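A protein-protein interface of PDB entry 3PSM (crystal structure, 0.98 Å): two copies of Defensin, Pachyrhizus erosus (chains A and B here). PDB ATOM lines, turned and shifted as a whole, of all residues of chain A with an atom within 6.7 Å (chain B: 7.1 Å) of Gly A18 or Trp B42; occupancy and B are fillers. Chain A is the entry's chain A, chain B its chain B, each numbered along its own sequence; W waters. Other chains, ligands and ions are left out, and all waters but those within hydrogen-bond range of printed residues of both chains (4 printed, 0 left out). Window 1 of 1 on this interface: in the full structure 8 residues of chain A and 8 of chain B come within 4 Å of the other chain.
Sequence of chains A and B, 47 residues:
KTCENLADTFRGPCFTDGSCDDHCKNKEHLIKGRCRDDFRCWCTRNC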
ATOM      1  N   PHE A  15      -3.068 -27.776  29.617  1.00  0.00           N
ATOM      2  CA  PHE A  15      -4.147 -28.590  29.077  1.00  0.00           C
ATOM      3  C   PHE A  15      -4.838 -27.961  27.897  1.00  0.00           C
ATOM      4  O   PHE A  15      -5.386 -28.673  27.084  1.00  0.00           O
ATOM      5  CB  PHE A  15      -5.187 -28.883  30.160  1.00  0.00           C
ATOM      6  CG  PHE A  15      -4.673 -29.752  31.271  1.00  0.00           C
ATOM      7  CD1 PHE A  15      -4.603 -29.267  32.568  1.00  0.00           C
ATOM      8  CD2 PHE A  15      -4.245 -31.044  31.061  1.00  0.00           C
ATOM      9  CE1 PHE A  15      -4.147 -30.073  33.610  1.00  0.00           C
ATOM     10  CE2 PHE A  15      -3.795 -31.808  32.107  1.00  0.00           C
ATOM     11  CZ  PHE A  15      -3.727 -31.355  33.374  1.00  0.00           C
ATOM     12  N   THR A  16      -4.890 -26.640  27.821  1.00  0.00           N
ATOM     13  CA  THR A  16      -5.604 -25.928  26.768  1.00  0.00           C
ATOM     14  C   THR A  16      -4.653 -24.983  26.076  1.00  0.00           C
ATOM     15  O   THR A  16      -3.937 -24.214  26.726  1.00  0.00           O
ATOM     16  CB  THR A  16      -6.864 -25.226  27.273  1.00  0.00           C
ATOM     17  OG1 THR A  16      -6.487 -24.065  28.018  1.00  0.00           O
ATOM     18  CG2 THR A  16      -7.732 -26.180  28.093  1.00  0.00           C
ATOM     19  N   ASP A  17      -4.675 -25.011  24.734  1.00  0.00           N
ATOM     20  CA  ASP A  17      -3.871 -24.030  24.011  1.00  0.00           C
ATOM     21  C   ASP A  17      -4.336 -22.630  24.302  1.00  0.00           C
ATOM     22  O   ASP A  17      -3.494 -21.706  24.364  1.00  0.00           O
ATOM     23  CB  ASP A  17      -3.917 -24.304  22.513  1.00  0.00           C
ATOM     24  CG  ASP A  17      -3.012 -25.484  22.143  1.00  0.00           C
ATOM     25  OD1 ASP A  17      -2.326 -26.059  22.937  1.00  0.00           O
ATOM     26  OD2 ASP A  17      -2.942 -25.752  20.900  1.00  0.00           O
ATOM     27  N   GLY A  18      -5.636 -22.393  24.510  1.00  0.00           N
ATOM     28  CA  GLY A  18      -6.066 -21.043  24.821  1.00  0.00           C
ATOM     29  C   GLY A  18      -5.455 -20.499  26.064  1.00  0.00           C
ATOM     30  O   GLY A  18      -5.051 -19.337  26.144  1.00  0.00           O
ATOM     31  N   SER A  19      -5.317 -21.323  27.135  1.00  0.00           N
ATOM     32  CA  SER A  19      -4.708 -20.839  28.360  1.00  0.00           C
ATOM     33  C   SER A  19      -3.241 -20.402  28.103  1.00  0.00           C
ATOM     34  O   SER A  19      -2.781 -19.386  28.651  1.00  0.00           O
ATOM     35  CB  SER A  19      -4.736 -21.869  29.463  1.00  0.00           C
ATOM     36  OG  SER A  19      -3.929 -23.012  29.215  1.00  0.00           O
ATOM     37  N   CYS A  20      -2.527 -21.163  27.293  1.00  0.00           N
ATOM     38  CA  CYS A  20      -1.138 -20.842  27.012  1.00  0.00           C
ATOM     39  C   CYS A  20      -0.991 -19.672  26.092  1.00  0.00           C
ATOM     40  O   CYS A  20      -0.136 -18.792  26.295  1.00  0.00           O
ATOM     41  CB  CYS A  20      -0.454 -22.087  26.437  1.00  0.00           C
ATOM     42  SG  CYS A  20       1.279 -21.873  26.025  1.00  0.00           S
ATOM     43  N   ASP A  21      -1.823 -19.608  25.055  1.00  0.00           N
ATOM     44  CA  ASP A  21      -1.795 -18.458  24.139  1.00  0.00           C
ATOM     45  C   ASP A  21      -2.097 -17.170  24.876  1.00  0.00           C
ATOM     46  O   ASP A  21      -1.456 -16.140  24.652  1.00  0.00           O
ATOM     47  CB  ASP A  21      -2.778 -18.712  23.004  1.00  0.00           C
ATOM     48  CG  ASP A  21      -2.553 -17.890  21.764  1.00  0.00           C
ATOM     49  OD1 ASP A  21      -1.390 -17.605  21.430  1.00  0.00           O
ATOM     50  OD2 ASP A  21      -3.571 -17.539  21.115  1.00  0.00           O
ATOM     51  N   ASP A  22      -3.067 -17.208  25.794  1.00  0.00           N
ATOM     52  CA  ASP A  22      -3.385 -16.071  26.642  1.00  0.00           C
ATOM     53  C   ASP A  22      -2.157 -15.640  27.430  1.00  0.00           C
ATOM     54  O   ASP A  22      -1.729 -14.489  27.414  1.00  0.00           O
ATOM     55  CB  ASP A  22      -4.553 -16.457  27.561  1.00  0.00           C
ATOM     56  CG  ASP A  22      -4.905 -15.501  28.663  1.00  0.00           C
ATOM     57  OD1 ASP A  22      -4.549 -14.312  28.562  1.00  0.00           O
ATOM     58  OD2 ASP A  22      -5.503 -15.956  29.674  1.00  0.00           O
ATOM     59  N   HIS A  23      -1.547 -16.609  28.156  1.00  0.00           N
ATOM     60  CA  HIS A  23      -0.353 -16.297  28.918  1.00  0.00           C
ATOM     61  C   HIS A  23       0.720 -15.659  28.045  1.00  0.00           C
ATOM     62  O   HIS A  23       1.326 -14.624  28.379  1.00  0.00           O
ATOM     63  CB  HIS A  23       0.175 -17.588  29.592  1.00  0.00           C
ATOM     64  CG  HIS A  23       1.508 -17.330  30.271  1.00  0.00           C
ATOM     65  ND1 HIS A  23       1.564 -16.936  31.600  1.00  0.00           N
ATOM     66  CD2 HIS A  23       2.764 -17.394  29.754  1.00  0.00           C
ATOM     67  CE1 HIS A  23       2.848 -16.742  31.852  1.00  0.00           C
ATOM     68  NE2 HIS A  23       3.574 -16.986  30.780  1.00  0.00           N
ATOM     69  N   LYS A  25       0.669 -14.256  25.024  1.00  0.00           N
ATOM     70  CA  LYS A  25       0.327 -12.967  24.422  1.00  0.00           C
ATOM     71  C   LYS A  25       0.212 -11.872  25.467  1.00  0.00           C
ATOM     72  O   LYS A  25       0.642 -10.730  25.229  1.00  0.00           O
ATOM     73  CB  LYS A  25      -0.972 -13.079  23.631  1.00  0.00           C
ATOM     74  CG  LYS A  25      -0.856 -13.824  22.340  1.00  0.00           C
ATOM     75  CD  LYS A  25      -2.183 -14.089  21.663  1.00  0.00           C
ATOM     76  CE  LYS A  25      -1.994 -14.573  20.221  1.00  0.00           C
ATOM     77  NZ  LYS A  25      -3.182 -15.178  19.644  1.00  0.00           N
ATOM     78  N   ASN A  26      -0.443 -12.161  26.576  1.00  0.00           N
ATOM     79  CA  ASN A  26      -0.903 -11.122  27.510  1.00  0.00           C
ATOM     80  C   ASN A  26      -0.076 -10.961  28.734  1.00  0.00           C
ATOM     81  O   ASN A  26      -0.130  -9.871  29.346  1.00  0.00           O
ATOM     82  CB  ASN A  26      -2.371 -11.397  27.883  1.00  0.00           C
ATOM     83  CG  ASN A  26      -3.236 -11.359  26.656  1.00  0.00           C
ATOM     84  OD1 ASN A  26      -3.114 -10.408  25.839  1.00  0.00           O
ATOM     85  ND2 ASN A  26      -4.101 -12.329  26.495  1.00  0.00           N
ATOM     86  N   GLY A  33       1.171 -18.744  22.011  1.00  0.00           N
ATOM     87  CA  GLY A  33       1.502 -19.880  22.829  1.00  0.00           C
ATOM     88  C   GLY A  33       0.674 -21.097  22.470  1.00  0.00           C
ATOM     89  O   GLY A  33      -0.453 -20.976  21.993  1.00  0.00           O
ATOM     90  N   ARG A  34       1.223 -22.261  22.800  1.00  0.00           N
ATOM     91  CA  ARG A  34       0.515 -23.518  22.665  1.00  0.00           C
ATOM     92  C   ARG A  34       1.041 -24.502  23.702  1.00  0.00           C
ATOM     93  O   ARG A  34       2.220 -24.433  24.094  1.00  0.00           O
ATOM     94  CB  ARG A  34       0.649 -24.129  21.282  1.00  0.00           C
ATOM     95  CG  ARG A  34       2.102 -24.477  20.952  1.00  0.00           C
ATOM     96  CD  ARG A  34       2.219 -25.266  19.690  1.00  0.00           C
ATOM     97  NE  ARG A  34       3.621 -25.492  19.362  1.00  0.00           N
ATOM     98  CZ  ARG A  34       4.044 -26.425  18.518  1.00  0.00           C
ATOM     99  NH1 ARG A  34       3.187 -27.246  17.933  1.00  0.00           N
ATOM    100  NH2 ARG A  34       5.359 -26.461  18.326  1.00  0.00           N
ATOM    101  N   CYS A  35       0.208 -25.444  24.085  1.00  0.00           N
ATOM    102  CA  CYS A  35       0.758 -26.613  24.815  1.00  0.00           C
ATOM    103  C   CYS A  35       1.453 -27.532  23.831  1.00  0.00           C
ATOM    104  O   CYS A  35       1.065 -27.667  22.684  1.00  0.00           O
ATOM    105  CB  CYS A  35      -0.353 -27.409  25.470  1.00  0.00           C
ATOM    106  SG  CYS A  35      -1.495 -26.443  26.513  1.00  0.00           S
ATOM    107  N   GLU B   4      -5.632 -12.225  17.160  1.00  0.00           N
ATOM    108  CA  GLU B   4      -6.675 -12.936  17.884  1.00  0.00           C
ATOM    109  C   GLU B   4      -6.348 -12.854  19.371  1.00  0.00           C
ATOM    110  O   GLU B   4      -5.222 -13.183  19.779  1.00  0.00           O
ATOM    111  CB  GLU B   4      -6.740 -14.389  17.413  1.00  0.00           C
ATOM    112  CG  GLU B   4      -7.844 -15.169  18.103  1.00  0.00           C
ATOM    113  CD  GLU B   4      -8.103 -16.534  17.525  1.00  0.00           C
ATOM    114  OE1 GLU B   4      -7.141 -17.320  17.326  1.00  0.00           O
ATOM    115  OE2 GLU B   4      -9.273 -16.858  17.236  1.00  0.00           O
ATOM    116  N   ASN B   5      -7.320 -12.446  20.170  1.00  0.00           N
ATOM    117  CA  ASN B   5      -7.090 -12.338  21.620  1.00  0.00           C
ATOM    118  C   ASN B   5      -8.428 -12.474  22.304  1.00  0.00           C
ATOM    119  O   ASN B   5      -9.461 -12.574  21.664  1.00  0.00           O
ATOM    120  CB  ASN B   5      -6.312 -11.041  21.946  1.00  0.00           C
ATOM    121  CG  ASN B   5      -5.476 -11.167  23.174  1.00  0.00           C
ATOM    122  OD1 ASN B   5      -5.765 -11.890  24.136  1.00  0.00           O
ATOM    123  ND2 ASN B   5      -4.350 -10.444  23.204  1.00  0.00           N
ATOM    124  N   LEU B   6      -8.402 -12.488  23.628  1.00  0.00           N
ATOM    125  CA  LEU B   6      -9.604 -12.703  24.417  1.00  0.00           C
ATOM    126  C   LEU B   6     -10.590 -11.574  24.191  1.00  0.00           C
ATOM    127  O   LEU B   6     -10.227 -10.397  24.078  1.00  0.00           O
ATOM    128  CB  LEU B   6      -9.232 -12.776  25.867  1.00  0.00           C
ATOM    129  CG  LEU B   6      -8.580 -14.096  26.319  1.00  0.00           C
ATOM    130  CD1 LEU B   6      -7.906 -13.944  27.659  1.00  0.00           C
ATOM    131  CD2 LEU B   6      -9.613 -15.218  26.337  1.00  0.00           C
ATOM    132  N   ALA B   7     -11.865 -11.949  24.185  1.00  0.00           N
ATOM    133  CA  ALA B   7     -12.949 -10.977  24.239  1.00  0.00           C
ATOM    134  C   ALA B   7     -12.842 -10.143  25.513  1.00  0.00           C
ATOM    135  O   ALA B   7     -12.335 -10.579  26.543  1.00  0.00           O
ATOM    136  CB  ALA B   7     -14.267 -11.674  24.185  1.00  0.00           C
ATOM    137  N   PHE B  10     -17.059 -10.614  27.690  1.00  0.00           N
ATOM    138  CA  PHE B  10     -17.942 -11.691  27.308  1.00  0.00           C
ATOM    139  C   PHE B  10     -18.199 -12.465  28.598  1.00  0.00           C
ATOM    140  O   PHE B  10     -17.278 -12.995  29.216  1.00  0.00           O
ATOM    141  CB  PHE B  10     -17.293 -12.604  26.262  1.00  0.00           C
ATOM    142  CG  PHE B  10     -18.113 -13.799  25.892  1.00  0.00           C
ATOM    143  CD1 PHE B  10     -18.947 -13.727  24.790  1.00  0.00           C
ATOM    144  CD2 PHE B  10     -18.072 -14.996  26.532  1.00  0.00           C
ATOM    145  CE1 PHE B  10     -19.726 -14.796  24.380  1.00  0.00           C
ATOM    146  CE2 PHE B  10     -18.833 -16.060  26.159  1.00  0.00           C
ATOM    147  CZ  PHE B  10     -19.662 -15.961  25.079  1.00  0.00           C
ATOM    148  N   CYS B  14     -17.769 -20.001  27.191  1.00  0.00           N
ATOM    149  CA  CYS B  14     -17.946 -19.994  25.751  1.00  0.00           C
ATOM    150  C   CYS B  14     -18.114 -21.442  25.285  1.00  0.00           C
ATOM    151  O   CYS B  14     -17.162 -22.162  25.097  1.00  0.00           O
ATOM    152  CB  CYS B  14     -16.737 -19.356  25.088  1.00  0.00           C
ATOM    153  SG  CYS B  14     -17.001 -18.731  23.416  1.00  0.00           S
ATOM    154  N   CYS B  20     -20.033 -16.198  20.670  1.00  0.00           N
ATOM    155  CA  CYS B  20     -18.785 -15.431  20.641  1.00  0.00           C
ATOM    156  C   CYS B  20     -18.631 -14.590  19.412  1.00  0.00           C
ATOM    157  O   CYS B  20     -18.260 -13.438  19.463  1.00  0.00           O
ATOM    158  CB  CYS B  20     -17.639 -16.418  20.818  1.00  0.00           C
ATOM    159  SG  CYS B  20     -16.016 -15.641  20.793  1.00  0.00           S
ATOM    160  N   ASP B  21     -18.891 -15.211  18.239  1.00  0.00           N
ATOM    161  CA  ASP B  21     -18.836 -14.422  16.988  1.00  0.00           C
ATOM    162  C   ASP B  21     -19.735 -13.190  17.073  1.00  0.00           C
ATOM    163  O   ASP B  21     -19.345 -12.105  16.665  1.00  0.00           O
ATOM    164  CB  ASP B  21     -19.209 -15.339  15.811  1.00  0.00           C
ATOM    165  CG  ASP B  21     -18.925 -14.698  14.478  1.00  0.00           C
ATOM    166  OD1 ASP B  21     -17.803 -14.322  14.221  1.00  0.00           O
ATOM    167  OD2 ASP B  21     -19.954 -14.614  13.679  1.00  0.00           O
ATOM    168  N   CYS B  24     -18.161 -10.581  19.429  1.00  0.00           N
ATOM    169  CA  CYS B  24     -17.016  -9.947  18.820  1.00  0.00           C
ATOM    170  C   CYS B  24     -17.414  -8.972  17.715  1.00  0.00           C
ATOM    171  O   CYS B  24     -16.882  -7.875  17.655  1.00  0.00           O
ATOM    172  CB  CYS B  24     -16.055 -11.007  18.299  1.00  0.00           C
ATOM    173  SG  CYS B  24     -15.321 -12.017  19.617  1.00  0.00           S
ATOM    174  N   LYS B  32     -14.577 -11.158  13.852  1.00  0.00           N
ATOM    175  CA  LYS B  32     -15.207 -12.475  14.065  1.00  0.00           C
ATOM    176  C   LYS B  32     -14.770 -12.966  15.448  1.00  0.00           C
ATOM    177  O   LYS B  32     -13.865 -12.406  16.051  1.00  0.00           O
ATOM    178  CB  LYS B  32     -14.792 -13.473  12.996  1.00  0.00           C
ATOM    179  CG  LYS B  32     -13.295 -13.737  12.865  1.00  0.00           C
ATOM    180  CD  LYS B  32     -12.921 -14.669  11.717  1.00  0.00           C
ATOM    181  CE  LYS B  32     -11.433 -14.885  11.630  1.00  0.00           C
ATOM    182  NZ  LYS B  32     -11.040 -15.807  10.511  1.00  0.00           N
ATOM    183  N   GLY B  33     -15.420 -14.036  15.874  1.00  0.00           N
ATOM    184  CA  GLY B  33     -15.033 -14.680  17.137  1.00  0.00           C
ATOM    185  C   GLY B  33     -15.290 -16.168  17.095  1.00  0.00           C
ATOM    186  O   GLY B  33     -16.051 -16.662  16.262  1.00  0.00           O
ATOM    187  N   ARG B  34     -14.644 -16.866  18.030  1.00  0.00           N
ATOM    188  CA  ARG B  34     -14.845 -18.289  18.203  1.00  0.00           C
ATOM    189  C   ARG B  34     -14.544 -18.633  19.662  1.00  0.00           C
ATOM    190  O   ARG B  34     -13.696 -17.980  20.297  1.00  0.00           O
ATOM    191  CB  ARG B  34     -13.955 -19.117  17.267  1.00  0.00           C
ATOM    192  CG  ARG B  34     -12.469 -18.979  17.621  1.00  0.00           C
ATOM    193  CD  ARG B  34     -11.583 -19.592  16.563  1.00  0.00           C
ATOM    194  NE  ARG B  34     -10.175 -19.474  16.890  1.00  0.00           N
ATOM    195  CZ  ARG B  34      -9.326 -20.449  17.212  1.00  0.00           C
ATOM    196  NH1 ARG B  34      -9.685 -21.709  17.298  1.00  0.00           N
ATOM    197  NH2 ARG B  34      -8.081 -20.128  17.428  1.00  0.00           N
ATOM    198  N   CYS B  35     -15.170 -19.682  20.171  1.00  0.00           N
ATOM    199  CA  CYS B  35     -14.749 -20.265  21.436  1.00  0.00           C
ATOM    200  C   CYS B  35     -13.488 -21.114  21.212  1.00  0.00           C
ATOM    201  O   CYS B  35     -13.365 -21.778  20.207  1.00  0.00           O
ATOM    202  CB  CYS B  35     -15.836 -21.170  22.024  1.00  0.00           C
ATOM    203  SG  CYS B  35     -17.436 -20.361  22.258  1.00  0.00           S
ATOM    204  N   ARG B  36     -12.611 -21.123  22.186  1.00  0.00           N
ATOM    205  CA  ARG B  36     -11.446 -21.992  22.152  1.00  0.00           C
ATOM    206  C   ARG B  36     -11.519 -23.034  23.237  1.00  0.00           C
ATOM    207  O   ARG B  36     -12.493 -23.162  23.948  1.00  0.00           O
ATOM    208  CB  ARG B  36     -10.146 -21.141  22.199  1.00  0.00           C
ATOM    209  CG  ARG B  36      -9.966 -20.337  20.939  1.00  0.00           C
ATOM    210  CD  ARG B  36      -8.684 -19.561  20.930  1.00  0.00           C
ATOM    211  NE  ARG B  36      -7.540 -20.473  20.804  1.00  0.00           N
ATOM    212  CZ  ARG B  36      -6.288 -20.063  20.897  1.00  0.00           C
ATOM    213  NH1 ARG B  36      -6.023 -18.805  21.166  1.00  0.00           N
ATOM    214  NH2 ARG B  36      -5.309 -20.918  20.735  1.00  0.00           N
ATOM    215  N   ASP B  37     -10.471 -23.862  23.303  1.00  0.00           N
ATOM    216  CA  ASP B  37     -10.417 -25.008  24.207  1.00  0.00           C
ATOM    217  C   ASP B  37     -10.317 -24.625  25.656  1.00  0.00           C
ATOM    218  O   ASP B  37     -10.470 -25.508  26.525  1.00  0.00           O
ATOM    219  CB  ASP B  37      -9.306 -25.964  23.775  1.00  0.00           C
ATOM    220  CG  ASP B  37      -7.909 -25.408  23.806  1.00  0.00           C
ATOM    221  OD1 ASP B  37      -7.745 -24.187  24.032  1.00  0.00           O
ATOM    222  OD2 ASP B  37      -6.952 -26.228  23.604  1.00  0.00           O
ATOM    223  N   ASP B  38     -10.124 -23.358  25.963  1.00  0.00           N
ATOM    224  CA  ASP B  38     -10.228 -22.802  27.282  1.00  0.00           C
ATOM    225  C   ASP B  38     -11.667 -22.426  27.666  1.00  0.00           C
ATOM    226  O   ASP B  38     -11.940 -21.926  28.758  1.00  0.00           O
ATOM    227  CB  ASP B  38      -9.296 -21.597  27.444  1.00  0.00           C
ATOM    228  CG  ASP B  38      -9.562 -20.502  26.430  1.00  0.00           C
ATOM    229  OD1 ASP B  38     -10.446 -20.628  25.565  1.00  0.00           O
ATOM    230  OD2 ASP B  38      -8.827 -19.479  26.570  1.00  0.00           O
ATOM    231  N   PHE B  39     -12.609 -22.624  26.750  1.00  0.00           N
ATOM    232  CA  PHE B  39     -13.997 -22.219  26.933  1.00  0.00           C
ATOM    233  C   PHE B  39     -14.136 -20.733  27.198  1.00  0.00           C
ATOM    234  O   PHE B  39     -15.040 -20.277  27.898  1.00  0.00           O
ATOM    235  CB  PHE B  39     -14.737 -23.082  27.992  1.00  0.00           C
ATOM    236  CG  PHE B  39     -14.567 -24.554  27.643  1.00  0.00           C
ATOM    237  CD1 PHE B  39     -13.886 -25.394  28.500  1.00  0.00           C
ATOM    238  CD2 PHE B  39     -15.067 -25.033  26.429  1.00  0.00           C
ATOM    239  CE1 PHE B  39     -13.704 -26.726  28.127  1.00  0.00           C
ATOM    240  CE2 PHE B  39     -14.901 -26.357  26.038  1.00  0.00           C
ATOM    241  CZ  PHE B  39     -14.197 -27.146  26.898  1.00  0.00           C
ATOM    242  N   ARG B  40     -13.264 -19.959  26.558  1.00  0.00           N
ATOM    243  CA  ARG B  40     -13.363 -18.512  26.496  1.00  0.00           C
ATOM    244  C   ARG B  40     -13.620 -18.098  25.070  1.00  0.00           C
ATOM    245  O   ARG B  40     -13.342 -18.812  24.099  1.00  0.00           O
ATOM    246  CB  ARG B  40     -12.137 -17.856  27.111  1.00  0.00           C
ATOM    247  CG  ARG B  40     -12.078 -18.127  28.622  1.00  0.00           C
ATOM    248  CD  ARG B  40     -10.926 -17.398  29.258  1.00  0.00           C
ATOM    249  NE  ARG B  40      -9.659 -17.887  28.861  1.00  0.00           N
ATOM    250  CZ  ARG B  40      -8.473 -17.538  29.293  1.00  0.00           C
ATOM    251  NH1 ARG B  40      -8.319 -16.633  30.273  1.00  0.00           N
ATOM    252  NH2 ARG B  40      -7.307 -18.014  28.915  1.00  0.00           N
ATOM    253  N   CYS B  41     -14.162 -16.884  24.917  1.00  0.00           N
ATOM    254  CA  CYS B  41     -14.428 -16.242  23.632  1.00  0.00           C
ATOM    255  C   CYS B  41     -13.211 -15.451  23.207  1.00  0.00           C
ATOM    256  O   CYS B  41     -12.698 -14.645  23.973  1.00  0.00           O
ATOM    257  CB  CYS B  41     -15.646 -15.341  23.776  1.00  0.00           C
ATOM    258  SG  CYS B  41     -16.021 -14.322  22.340  1.00  0.00           S
ATOM    259  N   TRP B  42     -12.762 -15.726  21.975  1.00  0.00           N
ATOM    260  CA  TRP B  42     -11.630 -15.062  21.371  1.00  0.00           C
ATOM    261  C   TRP B  42     -12.069 -14.330  20.116  1.00  0.00           C
ATOM    262  O   TRP B  42     -12.713 -14.925  19.231  1.00  0.00           O
ATOM    263  CB  TRP B  42     -10.536 -16.088  21.024  1.00  0.00           C
ATOM    264  CG  TRP B  42      -9.871 -16.704  22.214  1.00  0.00           C
ATOM    265  CD1 TRP B  42     -10.405 -17.576  23.108  1.00  0.00           C
ATOM    266  CD2 TRP B  42      -8.506 -16.475  22.610  1.00  0.00           C
ATOM    267  NE1 TRP B  42      -9.464 -17.913  24.002  1.00  0.00           N
ATOM    268  CE2 TRP B  42      -8.272 -17.256  23.754  1.00  0.00           C
ATOM    269  CE3 TRP B  42      -7.454 -15.706  22.090  1.00  0.00           C
ATOM    270  CZ2 TRP B  42      -7.041 -17.281  24.392  1.00  0.00           C
ATOM    271  CZ3 TRP B  42      -6.250 -15.738  22.736  1.00  0.00           C
ATOM    272  CH2 TRP B  42      -6.039 -16.529  23.884  1.00  0.00           C
ATOM    273  N   CYS B  43     -11.731 -13.057  20.035  1.00  0.00           N
ATOM    274  CA  CYS B  43     -12.063 -12.223  18.886  1.00  0.00           C
ATOM    275  C   CYS B  43     -10.848 -12.023  17.998  1.00  0.00           C
ATOM    276  O   CYS B  43      -9.723 -11.895  18.491  1.00  0.00           O
ATOM    277  CB  CYS B  43     -12.543 -10.827  19.321  1.00  0.00           C
ATOM    278  SG  CYS B  43     -13.945 -10.765  20.452  1.00  0.00           S
ATOM    279  N   THR B  44     -11.095 -11.906  16.696  1.00  0.00           N
ATOM    280  CA  THR B  44     -10.092 -11.496  15.730  1.00  0.00           C
ATOM    281  C   THR B  44     -10.375 -10.072  15.280  1.00  0.00           C
ATOM    282  O   THR B  44     -11.512  -9.722  15.042  1.00  0.00           O
ATOM    283  CB  THR B  44     -10.107 -12.430  14.509  1.00  0.00           C
ATOM    284  OG1 THR B  44      -9.790 -13.757  14.986  1.00  0.00           O
ATOM    285  CG2 THR B  44      -9.078 -12.051  13.464  1.00  0.00           C
HETATM  286  O   HOH W   1      -4.498 -17.187  18.016  1.00  0.00           O
HETATM  287  O   HOH W   2      -2.870 -13.229  16.886  1.00  0.00           O
HETATM  288  O   HOH W   3      -2.478 -21.017  20.236  1.00  0.00           O
HETATM  289  O   HOH W   4      -6.189  -9.390  26.296  1.00  0.00           O
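Positions printed for both chains: 20, 21, 33, 34 and 35.
OD1 of Asp A22 lies within hydrogen-bond range of ND2 of Asn A26 (2.9 Å).
The side-chain carboxylate (OE2) of Glu B4 is in salt-bridge range of the guanidinium group (NE) of Arg B34 (2.8 Å).
The backbone carbonyl oxygen (O) of Asn B5 is in hydrogen-bond range of the backbone NH (N) of Cys B43, 2.8 Å away.
The backbone carbonyl oxygen of Arg B34 sits at hydrogen-bond distance from the backbone NH of Trp B42, 3.0 Å away.
The side-chain sulfur (SG) of Cys B20 is disulfide-bonded to the side-chain sulfur (SG) of Cys B41 (2.0 Å).
The side-chain sulfur (SG) of Cys B43 is disulfide-bonded to the side-chain sulfur (SG) of Cys B24 (2.0 Å).
Among the printed residues, merely in contact across the chains: Thr A16 with Asp B37 (3.2 Å), Gly A18 with Trp B42 (3.4 Å), Asp A22 with Leu B6 (3.5 Å), Gly A18 with Asp B38 (3.6 Å), Asp A22 with Trp B42 (3.6 Å), Asp A21 with Trp B42 (3.6 Å), Thr A16 with Asp B38 (3.8 Å), Gly A18 with Arg B40 (3.8 Å) and Ser A19 with Arg B40 (3.9 Å).
Printed residues of chain B that touch a printed residue of chain A: Glu B4, Asn B5, Leu B6, Arg B36, Asp B37, Asp B38, Arg B40 and Trp B42.
Hydrophobic or aromatic side chains of chain B that line the printed part of chain A: Leu B6 and Trp B42.
Printed residues of chain A that touch a printed residue of chain B: Thr A16, Asp A17, Gly A18, Ser A19, Asp A21, Asp A22, Lys A25 and Asn A26.
Among the printed residues, 15 pairs touch across the chains.
Among the printed residues, Asp or Glu carboxylates within 4 Å of a Lys or Arg side-chain nitrogen of the other chain: Asp A21 with Arg B36 (2.8 Å) and Asp A22 with Arg B40 (2.8 Å).
Of the printed residues of chain B, Thr A16 touches Asp B37 (3.2 Å) and Asp B38 (3.8 Å).
Printed residues of chain B within 4 Å of Gly A18: Asp B37 (2.8 Å), Asp B38 (3.6 Å), Arg B40 (3.8 Å) and Trp B42 (3.4 Å).
Cys A20 touches none of the printed residues of chain B.
Of the printed residues of chain B, Asp A22 touches Leu B6 (3.5 Å), Arg B40 (2.8 Å) and Trp B42 (3.6 Å).
Of the printed residues of chain A, Asp B37 touches Thr A16 (3.2 Å), Asp A17 (2.8 Å) and Gly A18 (2.8 Å).
Printed residues of chain A within 4 Å of Asp B38: Thr A16 (3.8 Å) and Gly A18 (3.6 Å).
Of the printed residues of chain A, Arg B40 touches Gly A18 (3.8 Å), Ser A19 (3.9 Å) and Asp A22 (2.8 Å).
Trp B42 touches just these residues of chain A: Gly A18 (3.4 Å), Asp A21 (3.6 Å) and Asp A22 (3.6 Å).
The nearest printed residue of chain B that does not touch Gly A18 is Arg B36 (4.1 Å).
The nearest residue of chain A that does not touch Trp B42 is Lys A25 (4.4 Å).
OD2 of Asp B37 lies within hydrogen-bond range of N of Asp A17, at 2.8 Å.
N of Gly A18 lies within hydrogen-bond range of OD1 of Asp B37 (2.8 Å).
The guanidinium group (NH1) of Arg B36 is in salt-bridge range of the side-chain carboxylate (OD2) of Asp A21.
OD2 of Asp A22 lies within salt-bridge range of NH2 of Arg B40 (2.8 Å).
O of Glu B4 sits at hydrogen-bond distance from NZ of Lys A25, 2.9 Å away.
The side-chain amide oxygen of Asn A26 sits at hydrogen-bond distance from the side-chain amide nitrogen of Asn B5 (2.9 Å).
Water W3 lies within hydrogen-bond range of the backbone carbonyl oxygen of Gly A33 (2.7 Å) and the guanidinium group of Arg B36 (2.9 Å).
Water W1 lies within hydrogen-bond range of OE1 of Glu B4 (2.7 Å), NZ of Lys A25 (2.9 Å) and OD2 of Asp A21 (3.3 Å).
Water W2 lies within hydrogen-bond range of the backbone NH (N) of Glu B4 (3.0 Å) and the side-chain amino group (NZ) of Lys A25 (3.4 Å).
Water W4 lies within hydrogen-bond range of OD1 of Asn A26 (3.3 Å) and OD1 of Asn B5 (3.3 Å).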
